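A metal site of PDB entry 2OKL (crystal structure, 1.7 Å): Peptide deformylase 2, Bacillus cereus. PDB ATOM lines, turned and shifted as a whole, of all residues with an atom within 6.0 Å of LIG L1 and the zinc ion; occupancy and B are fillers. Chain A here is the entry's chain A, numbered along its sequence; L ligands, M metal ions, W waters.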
ATOM      1  N   ARG A  57       1.896  -6.760  -8.980  1.00  0.00           N
ATOM      2  CA  ARG A  57       2.687  -7.078 -10.154  1.00  0.00           C
ATOM      3  C   ARG A  57       3.012  -5.711 -10.768  1.00  0.00           C
ATOM      4  O   ARG A  57       2.122  -4.903 -11.018  1.00  0.00           O
ATOM      5  CB  ARG A  57       1.878  -7.926 -11.133  1.00  0.00           C
ATOM      6  CG  ARG A  57       2.595  -8.288 -12.439  1.00  0.00           C
ATOM      7  CD  ARG A  57       1.713  -9.190 -13.312  1.00  0.00           C
ATOM      8  NE  ARG A  57       2.190  -9.281 -14.690  1.00  0.00           N
ATOM      9  CZ  ARG A  57       1.509  -9.866 -15.677  1.00  0.00           C
ATOM     10  NH1 ARG A  57       0.322 -10.430 -15.442  1.00  0.00           N
ATOM     11  NH2 ARG A  57       2.005  -9.884 -16.904  1.00  0.00           N
ATOM     12  N   PRO A  58       4.300  -5.423 -10.984  1.00  0.00           N
ATOM     13  CA  PRO A  58       4.724  -4.153 -11.562  1.00  0.00           C
ATOM     14  C   PRO A  58       4.118  -3.938 -12.948  1.00  0.00           C
ATOM     15  O   PRO A  58       4.075  -4.866 -13.760  1.00  0.00           O
ATOM     16  CB  PRO A  58       6.244  -4.284 -11.619  1.00  0.00           C
ATOM     17  CG  PRO A  58       6.548  -5.192 -10.465  1.00  0.00           C
ATOM     18  CD  PRO A  58       5.472  -6.234 -10.595  1.00  0.00           C
ATOM     19  N   GLY A  59       3.650  -2.722 -13.194  1.00  0.00           N
ATOM     20  CA  GLY A  59       3.047  -2.385 -14.483  1.00  0.00           C
ATOM     21  C   GLY A  59       3.246  -0.904 -14.748  1.00  0.00           C
ATOM     22  O   GLY A  59       3.599  -0.155 -13.846  1.00  0.00           O
ATOM     23  N   ILE A  60       3.015  -0.481 -15.990  1.00  0.00           N
ATOM     24  CA  ILE A  60       3.208   0.931 -16.326  1.00  0.00           C
ATOM     25  C   ILE A  60       1.943   1.648 -16.763  1.00  0.00           C
ATOM     26  O   ILE A  60       2.006   2.761 -17.281  1.00  0.00           O
ATOM     27  CB  ILE A  60       4.294   1.072 -17.419  1.00  0.00           C
ATOM     28  CG1 ILE A  60       3.959   0.190 -18.614  1.00  0.00           C
ATOM     29  CG2 ILE A  60       5.652   0.689 -16.849  1.00  0.00           C
ATOM     30  CD1 ILE A  60       5.017   0.236 -19.719  1.00  0.00           C
ATOM     31  N   GLY A  61       0.795   1.029 -16.528  1.00  0.00           N
ATOM     32  CA  GLY A  61      -0.478   1.641 -16.894  1.00  0.00           C
ATOM     33  C   GLY A  61      -1.642   0.798 -16.421  1.00  0.00           C
ATOM     34  O   GLY A  61      -1.474  -0.375 -16.099  1.00  0.00           O
ATOM     35  N   LEU A  62      -2.823   1.408 -16.376  1.00  0.00           N
ATOM     36  CA  LEU A  62      -4.017   0.702 -15.937  1.00  0.00           C
ATOM     37  C   LEU A  62      -5.276   1.368 -16.485  1.00  0.00           C
ATOM     38  O   LEU A  62      -5.340   2.604 -16.591  1.00  0.00           O
ATOM     39  CB  LEU A  62      -4.069   0.658 -14.407  1.00  0.00           C
ATOM     40  CG  LEU A  62      -5.196  -0.181 -13.801  1.00  0.00           C
ATOM     41  CD1 LEU A  62      -4.952  -1.642 -14.101  1.00  0.00           C
ATOM     42  CD2 LEU A  62      -5.267   0.046 -12.304  1.00  0.00           C
ATOM     43  N   ALA A  63      -6.277   0.561 -16.822  1.00  0.00           N
ATOM     44  CA  ALA A  63      -7.541   1.069 -17.325  1.00  0.00           C
ATOM     45  C   ALA A  63      -8.640   0.672 -16.331  1.00  0.00           C
ATOM     46  O   ALA A  63      -8.594  -0.406 -15.743  1.00  0.00           O
ATOM     47  CB  ALA A  63      -7.835   0.485 -18.703  1.00  0.00           C
ATOM     48  N   GLN A  66     -10.313  -2.766 -16.101  1.00  0.00           N
ATOM     49  CA  GLN A  66      -9.462  -3.774 -15.483  1.00  0.00           C
ATOM     50  C   GLN A  66      -9.723  -3.969 -13.986  1.00  0.00           C
ATOM     51  O   GLN A  66      -9.423  -5.023 -13.444  1.00  0.00           O
ATOM     52  CB  GLN A  66      -7.990  -3.441 -15.697  1.00  0.00           C
ATOM     53  CG  GLN A  66      -7.524  -3.643 -17.112  1.00  0.00           C
ATOM     54  CD  GLN A  66      -6.050  -3.376 -17.276  1.00  0.00           C
ATOM     55  OE1 GLN A  66      -5.610  -2.227 -17.247  1.00  0.00           O
ATOM     56  NE2 GLN A  66      -5.270  -4.440 -17.442  1.00  0.00           N
ATOM     57  N   LEU A 105       7.087  -3.225 -29.693  1.00  0.00           N
ATOM     58  CA  LEU A 105       8.118  -3.763 -28.814  1.00  0.00           C
ATOM     59  C   LEU A 105       8.485  -5.140 -29.397  1.00  0.00           C
ATOM     60  O   LEU A 105       7.612  -5.981 -29.660  1.00  0.00           O
ATOM     61  CB  LEU A 105       7.563  -3.912 -27.390  1.00  0.00           C
ATOM     62  CG  LEU A 105       7.514  -2.650 -26.516  1.00  0.00           C
ATOM     63  CD1 LEU A 105       6.458  -2.769 -25.423  1.00  0.00           C
ATOM     64  CD2 LEU A 105       8.893  -2.451 -25.894  1.00  0.00           C
ATOM     65  N   GLY A 107       9.853  -7.527 -27.930  1.00  0.00           N
ATOM     66  CA  GLY A 107       9.585  -8.556 -26.950  1.00  0.00           C
ATOM     67  C   GLY A 107       8.100  -8.717 -26.671  1.00  0.00           C
ATOM     68  O   GLY A 107       7.709  -9.451 -25.753  1.00  0.00           O
ATOM     69  N   GLY A 108       7.274  -8.039 -27.464  1.00  0.00           N
ATOM     70  CA  GLY A 108       5.830  -8.126 -27.305  1.00  0.00           C
ATOM     71  C   GLY A 108       5.255  -7.310 -26.159  1.00  0.00           C
ATOM     72  O   GLY A 108       5.917  -6.419 -25.615  1.00  0.00           O
ATOM     73  N   GLU A 109       4.019  -7.620 -25.783  1.00  0.00           N
ATOM     74  CA  GLU A 109       3.339  -6.937 -24.686  1.00  0.00           C
ATOM     75  C   GLU A 109       2.707  -7.909 -23.710  1.00  0.00           C
ATOM     76  O   GLU A 109       2.337  -9.029 -24.079  1.00  0.00           O
ATOM     77  CB  GLU A 109       2.244  -5.999 -25.240  1.00  0.00           C
ATOM     78  CG  GLU A 109       2.762  -4.716 -25.870  1.00  0.00           C
ATOM     79  CD  GLU A 109       1.634  -3.821 -26.379  1.00  0.00           C
ATOM     80  OE1 GLU A 109       0.531  -3.835 -25.776  1.00  0.00           O
ATOM     81  OE2 GLU A 109       1.847  -3.089 -27.364  1.00  0.00           O
ATOM     82  N   GLY A 110       2.583  -7.478 -22.465  1.00  0.00           N
ATOM     83  CA  GLY A 110       1.962  -8.276 -21.425  1.00  0.00           C
ATOM     84  C   GLY A 110       0.802  -7.447 -20.888  1.00  0.00           C
ATOM     85  O   GLY A 110       0.751  -6.242 -21.136  1.00  0.00           O
ATOM     86  N   CYS A 111      -0.120  -8.073 -20.160  1.00  0.00           N
ATOM     87  CA  CYS A 111      -1.276  -7.362 -19.622  1.00  0.00           C
ATOM     88  C   CYS A 111      -1.611  -7.908 -18.239  1.00  0.00           C
ATOM     89  O   CYS A 111      -1.577  -9.118 -18.008  1.00  0.00           O
ATOM     90  CB  CYS A 111      -2.488  -7.531 -20.569  1.00  0.00           C
ATOM     91  SG  CYS A 111      -4.014  -6.641 -20.112  1.00  0.00           S
ATOM     92  N   LEU A 112      -1.919  -7.005 -17.312  1.00  0.00           N
ATOM     93  CA  LEU A 112      -2.271  -7.407 -15.959  1.00  0.00           C
ATOM     94  C   LEU A 112      -3.523  -8.270 -15.925  1.00  0.00           C
ATOM     95  O   LEU A 112      -3.710  -9.051 -14.990  1.00  0.00           O
ATOM     96  CB  LEU A 112      -2.474  -6.168 -15.088  1.00  0.00           C
ATOM     97  CG  LEU A 112      -1.301  -5.742 -14.189  1.00  0.00           C
ATOM     98  CD1 LEU A 112      -0.030  -5.556 -15.003  1.00  0.00           C
ATOM     99  CD2 LEU A 112      -1.680  -4.461 -13.463  1.00  0.00           C
ATOM    100  N   SER A 113      -4.377  -8.133 -16.936  1.00  0.00           N
ATOM    101  CA  SER A 113      -5.619  -8.901 -17.014  1.00  0.00           C
ATOM    102  C   SER A 113      -5.456 -10.238 -17.731  1.00  0.00           C
ATOM    103  O   SER A 113      -6.404 -11.017 -17.814  1.00  0.00           O
ATOM    104  CB  SER A 113      -6.690  -8.080 -17.752  1.00  0.00           C
ATOM    105  OG  SER A 113      -7.045  -6.912 -17.039  1.00  0.00           O
ATOM    106  N   ARG A 124       1.695  -0.876 -33.161  1.00  0.00           N
ATOM    107  CA  ARG A 124       1.162   0.344 -32.552  1.00  0.00           C
ATOM    108  C   ARG A 124       1.549   1.540 -33.406  1.00  0.00           C
ATOM    109  O   ARG A 124       2.574   1.509 -34.078  1.00  0.00           O
ATOM    110  CB  ARG A 124       1.767   0.561 -31.163  1.00  0.00           C
ATOM    111  CG  ARG A 124       1.478  -0.515 -30.143  1.00  0.00           C
ATOM    112  CD  ARG A 124       0.013  -0.558 -29.814  1.00  0.00           C
ATOM    113  NE  ARG A 124      -0.264  -1.452 -28.699  1.00  0.00           N
ATOM    114  CZ  ARG A 124      -1.494  -1.703 -28.261  1.00  0.00           C
ATOM    115  NH1 ARG A 124      -2.534  -1.140 -28.846  1.00  0.00           N
ATOM    116  NH2 ARG A 124      -1.682  -2.518 -27.238  1.00  0.00           N
ATOM    117  N   LEU A 147       7.532   4.340 -26.506  1.00  0.00           N
ATOM    118  CA  LEU A 147       6.897   3.587 -25.422  1.00  0.00           C
ATOM    119  C   LEU A 147       5.671   4.267 -24.821  1.00  0.00           C
ATOM    120  O   LEU A 147       4.672   3.608 -24.570  1.00  0.00           O
ATOM    121  CB  LEU A 147       7.918   3.266 -24.309  1.00  0.00           C
ATOM    122  CG  LEU A 147       7.388   2.330 -23.221  1.00  0.00           C
ATOM    123  CD1 LEU A 147       6.858   1.029 -23.850  1.00  0.00           C
ATOM    124  CD2 LEU A 147       8.510   2.021 -22.232  1.00  0.00           C
ATOM    125  N   ILE A 150       2.769   3.748 -26.977  1.00  0.00           N
ATOM    126  CA  ILE A 150       2.357   2.344 -26.929  1.00  0.00           C
ATOM    127  C   ILE A 150       1.491   2.083 -25.698  1.00  0.00           C
ATOM    128  O   ILE A 150       0.428   1.479 -25.798  1.00  0.00           O
ATOM    129  CB  ILE A 150       3.575   1.393 -26.907  1.00  0.00           C
ATOM    130  CG1 ILE A 150       4.250   1.416 -28.284  1.00  0.00           C
ATOM    131  CG2 ILE A 150       3.139  -0.034 -26.543  1.00  0.00           C
ATOM    132  CD1 ILE A 150       5.525   0.577 -28.391  1.00  0.00           C
ATOM    133  N   VAL A 151       1.932   2.563 -24.545  1.00  0.00           N
ATOM    134  CA  VAL A 151       1.175   2.361 -23.310  1.00  0.00           C
ATOM    135  C   VAL A 151      -0.208   3.032 -23.412  1.00  0.00           C
ATOM    136  O   VAL A 151      -1.206   2.452 -22.986  1.00  0.00           O
ATOM    137  CB  VAL A 151       1.934   2.924 -22.088  1.00  0.00           C
ATOM    138  CG1 VAL A 151       1.093   2.759 -20.813  1.00  0.00           C
ATOM    139  CG2 VAL A 151       3.266   2.216 -21.948  1.00  0.00           C
ATOM    140  N   HIS A 154      -2.497   0.877 -25.529  1.00  0.00           N
ATOM    141  CA  HIS A 154      -2.881  -0.327 -24.802  1.00  0.00           C
ATOM    142  C   HIS A 154      -3.994  -0.003 -23.805  1.00  0.00           C
ATOM    143  O   HIS A 154      -4.999  -0.727 -23.732  1.00  0.00           O
ATOM    144  CB  HIS A 154      -1.655  -0.894 -24.061  1.00  0.00           C
ATOM    145  CG  HIS A 154      -1.935  -2.124 -23.249  1.00  0.00           C
ATOM    146  ND1 HIS A 154      -1.458  -3.366 -23.599  1.00  0.00           N
ATOM    147  CD2 HIS A 154      -2.626  -2.303 -22.099  1.00  0.00           C
ATOM    148  CE1 HIS A 154      -1.838  -4.250 -22.696  1.00  0.00           C
ATOM    149  NE2 HIS A 154      -2.548  -3.635 -21.776  1.00  0.00           N
ATOM    150  N   GLU A 155      -3.835   1.078 -23.039  1.00  0.00           N
ATOM    151  CA  GLU A 155      -4.833   1.438 -22.044  1.00  0.00           C
ATOM    152  C   GLU A 155      -6.143   1.912 -22.658  1.00  0.00           C
ATOM    153  O   GLU A 155      -7.222   1.557 -22.175  1.00  0.00           O
ATOM    154  CB  GLU A 155      -4.306   2.518 -21.095  1.00  0.00           C
ATOM    155  CG  GLU A 155      -3.070   2.125 -20.291  1.00  0.00           C
ATOM    156  CD  GLU A 155      -3.130   0.724 -19.713  1.00  0.00           C
ATOM    157  OE1 GLU A 155      -4.242   0.168 -19.514  1.00  0.00           O
ATOM    158  OE2 GLU A 155      -2.048   0.168 -19.446  1.00  0.00           O
ATOM    159  N   HIS A 158      -8.294  -0.886 -23.934  1.00  0.00           N
ATOM    160  CA  HIS A 158      -9.083  -1.483 -22.868  1.00  0.00           C
ATOM    161  C   HIS A 158     -10.444  -0.817 -22.725  1.00  0.00           C
ATOM    162  O   HIS A 158     -11.438  -1.469 -22.398  1.00  0.00           O
ATOM    163  CB  HIS A 158      -8.350  -1.380 -21.527  1.00  0.00           C
ATOM    164  CG  HIS A 158      -7.408  -2.511 -21.260  1.00  0.00           C
ATOM    165  ND1 HIS A 158      -7.802  -3.834 -21.299  1.00  0.00           N
ATOM    166  CD2 HIS A 158      -6.102  -2.522 -20.915  1.00  0.00           C
ATOM    167  CE1 HIS A 158      -6.779  -4.603 -20.981  1.00  0.00           C
ATOM    168  NE2 HIS A 158      -5.728  -3.842 -20.749  1.00  0.00           N
ATOM    169  N   PHE A 164      -4.626  -6.586 -26.154  1.00  0.00           N
ATOM    170  CA  PHE A 164      -3.395  -6.493 -26.921  1.00  0.00           C
ATOM    171  C   PHE A 164      -3.216  -7.582 -27.966  1.00  0.00           C
ATOM    172  O   PHE A 164      -2.809  -7.310 -29.092  1.00  0.00           O
ATOM    173  CB  PHE A 164      -2.184  -6.429 -25.975  1.00  0.00           C
ATOM    174  CG  PHE A 164      -1.714  -7.770 -25.481  1.00  0.00           C
ATOM    175  CD1 PHE A 164      -0.784  -8.507 -26.209  1.00  0.00           C
ATOM    176  CD2 PHE A 164      -2.166  -8.273 -24.275  1.00  0.00           C
ATOM    177  CE1 PHE A 164      -0.314  -9.742 -25.736  1.00  0.00           C
ATOM    178  CE2 PHE A 164      -1.703  -9.506 -23.783  1.00  0.00           C
ATOM    179  CZ  PHE A 164      -0.778 -10.240 -24.524  1.00  0.00           C
HETATM  180  C1  LIG L   1      -0.396  -3.017 -17.681  1.00  0.00           C
HETATM  181  C2  LIG L   1      -1.808  -3.249 -18.248  1.00  0.00           C
HETATM  182  O1  LIG L   1      -2.202  -4.434 -18.309  1.00  0.00           O
HETATM  183  N1  LIG L   1      -2.535  -2.226 -18.660  1.00  0.00           N
HETATM  184  O2  LIG L   1      -3.665  -2.333 -19.120  1.00  0.00           O
HETATM  185  C3  LIG L   1       0.636  -3.331 -18.829  1.00  0.00           C
HETATM  186  C4  LIG L   1       2.096  -3.596 -18.381  1.00  0.00           C
HETATM  187  O3  LIG L   1       2.698  -2.872 -17.608  1.00  0.00           O
HETATM  188  C5  LIG L   1       0.610  -2.089 -19.800  1.00  0.00           C
HETATM  189  C6  LIG L   1       1.584  -2.340 -20.975  1.00  0.00           C
HETATM  190  C7  LIG L   1       1.610  -1.209 -21.971  1.00  0.00           C
HETATM  191  C8  LIG L   1       2.138  -1.686 -23.326  1.00  0.00           C
HETATM  192  C9  LIG L   1       3.618  -1.857 -23.373  1.00  0.00           C
HETATM  193  N2  LIG L   1       2.642  -4.686 -18.911  1.00  0.00           N
HETATM  194  C10 LIG L   1       4.027  -5.116 -18.777  1.00  0.00           C
HETATM  195  C11 LIG L   1       4.173  -6.495 -18.048  1.00  0.00           C
HETATM  196  C12 LIG L   1       3.247  -6.598 -16.844  1.00  0.00           C
HETATM  197  C13 LIG L   1       5.619  -6.661 -17.593  1.00  0.00           C
HETATM  198  C14 LIG L   1       4.601  -5.153 -20.209  1.00  0.00           C
HETATM  199  O4  LIG L   1       3.998  -5.768 -21.078  1.00  0.00           O
HETATM  200  N3  LIG L   1       5.748  -4.501 -20.468  1.00  0.00           N
HETATM  201  C15 LIG L   1       6.360  -4.480 -21.805  1.00  0.00           C
HETATM  202  C16 LIG L   1       6.552  -3.714 -19.474  1.00  0.00           C
HETATM  203  C17 LIG L   1       7.712  -3.207 -20.273  1.00  0.00           C
HETATM  204  C18 LIG L   1       7.305  -3.277 -21.719  1.00  0.00           C
HETATM  205  C19 LIG L   1       7.139  -5.757 -22.176  1.00  0.00           C
HETATM  206  O5  LIG L   1       7.528  -5.866 -23.382  1.00  0.00           O
HETATM  207  C1  LG2 L   2      17.967  -4.041 -29.859  1.00  0.00           C
HETATM  208  C2  LG2 L   2      18.156  -2.731 -30.605  1.00  0.00           C
HETATM  209  O1  LG2 L   2      18.365  -2.822 -31.827  1.00  0.00           O
HETATM  210  N1  LG2 L   2      18.125  -1.572 -29.972  1.00  0.00           N
HETATM  211  O2  LG2 L   2      18.270  -0.474 -30.512  1.00  0.00           O
HETATM  212  C3  LG2 L   2      16.492  -4.143 -29.281  1.00  0.00           C
HETATM  213  C4  LG2 L   2      16.247  -3.390 -27.940  1.00  0.00           C
HETATM  214  O3  LG2 L   2      17.004  -3.493 -26.968  1.00  0.00           O
HETATM  215  C5  LG2 L   2      16.281  -5.682 -29.059  1.00  0.00           C
HETATM  216  C6  LG2 L   2      14.883  -6.008 -28.495  1.00  0.00           C
HETATM  217  C7  LG2 L   2      14.727  -7.512 -28.298  1.00  0.00           C
HETATM  218  C8  LG2 L   2      13.763  -7.853 -27.172  1.00  0.00           C
HETATM  219  C9  LG2 L   2      13.350  -9.286 -27.175  1.00  0.00           C
HETATM  220  N2  LG2 L   2      15.150  -2.639 -27.898  1.00  0.00           N
HETATM  221  C10 LG2 L   2      14.648  -1.966 -26.691  1.00  0.00           C
HETATM  222  C11 LG2 L   2      13.845  -0.659 -26.954  1.00  0.00           C
HETATM  223  C12 LG2 L   2      13.004  -0.188 -25.780  1.00  0.00           C
HETATM  224  C13 LG2 L   2      12.971  -0.877 -28.187  1.00  0.00           C
HETATM  225  C14 LG2 L   2      13.845  -3.034 -25.877  1.00  0.00           C
HETATM  226  O4  LG2 L   2      12.955  -3.680 -26.433  1.00  0.00           O
HETATM  227  N3  LG2 L   2      14.173  -3.216 -24.588  1.00  0.00           N
HETATM  228  C15 LG2 L   2      13.499  -4.192 -23.734  1.00  0.00           C
HETATM  229  C16 LG2 L   2      15.247  -2.469 -23.842  1.00  0.00           C
HETATM  230  C17 LG2 L   2      15.204  -3.038 -22.444  1.00  0.00           C
HETATM  231  C18 LG2 L   2      14.445  -4.323 -22.527  1.00  0.00           C
HETATM  232  C19 LG2 L   2      12.100  -3.776 -23.293  1.00  0.00           C
HETATM  233  O5  LG2 L   2      11.376  -4.671 -22.776  1.00  0.00           O
HETATM  234 ZN    ZN M   1      -3.652  -4.314 -20.178  1.00  0.00          ZN
HETATM  235  O   HOH W   1      10.135  -6.695 -24.047  1.00  0.00           O
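The zinc ion is bound by NE2 of His 154, NE2 of His 158, O2 of LIG L1, SG of Cys 111 and O1 of LIG L1.
Merely in contact with the zinc ion: Gln 66.
Four residues have an atom within 4 Å of the zinc ion: Gln 66, Cys 111, His 154 and His 158.
Water W1 lies within hydrogen-bond range of an oxygen (O5) of LG2 L2 (2.7 Å) and an oxygen (O5) of LIG L1 (2.8 Å).
The side-chain carboxylate (OE1) of Glu 109 is in hydrogen-bond range of a ring nitrogen (ND1) of His 154, at 3.0 Å.
The side-chain amide nitrogen of Gln 66 lies close to a ring nitrogen (NE2) of His 158.
The guanidinium group (NH1) of Arg 57 lies within hydrogen-bond range of the backbone carbonyl oxygen (O) of Cys 111, 3.5 Å away.
SG of Cys 111 sits close to N of Ser 113, at 3.5 Å.
The side-chain carboxylate of Glu 155 is in hydrogen-bond range of the backbone NH of Leu 62 (3.4 Å).
OE1 of Glu 155 lies within hydrogen-bond range of N of Ala 63, 3.4 Å away.
The side-chain amide nitrogen (NE2) of Gln 66 is in hydrogen-bond range of the side-chain hydroxyl (OG) of Ser 113, 3.1 Å away.
The guanidinium group (NH2) of Arg 124 is in salt-bridge range of the side-chain carboxylate (OE1) of Glu 109.
Residues that only touch LIG L1: Arg 57 (3.5 Å), Pro 58 (3.6 Å), Gly 59 (3.2 Å), Leu 105 (3.6 Å), Glu 109 (3.6 Å), Ile 150 (3.7 Å) and Val 151 (3.8 Å).
Hydrophobic or aromatic side chains that line LIG L1: Ile 60, Leu 105, Leu 112, Ile 150, Val 151, His 154 and His 158.
Of the 24 residues printed, 17 come within 4 Å of LIG L1.
The side-chain carboxylate (OE2) of Glu 155 is in hydrogen-bond range of a nitrogen (N1) of LIG L1 (2.6 Å).
The backbone NH of Gly 110 lies within hydrogen-bond range of an oxygen (O4) of LIG L1, 2.6 Å away.
The backbone carbonyl oxygen (O) of Gly 110 lies within hydrogen-bond range of a nitrogen (N2) of LIG L1 (3.3 Å).
N1 of LIG L1 is in hydrogen-bond range of OE1 of Gln 66.
N of Leu 112 lies close to O1 of LIG L1, at 2.8 Å.
An oxygen (O5) of LIG L1 is in hydrogen-bond range of the backbone carbonyl oxygen (O) of Gly 108 (2.8 Å).
An oxygen (O3) of LIG L1 is in hydrogen-bond range of the backbone NH (N) of Ile 60, at 2.9 Å.
O of Gly 61 lies close to N1 of LIG L1.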
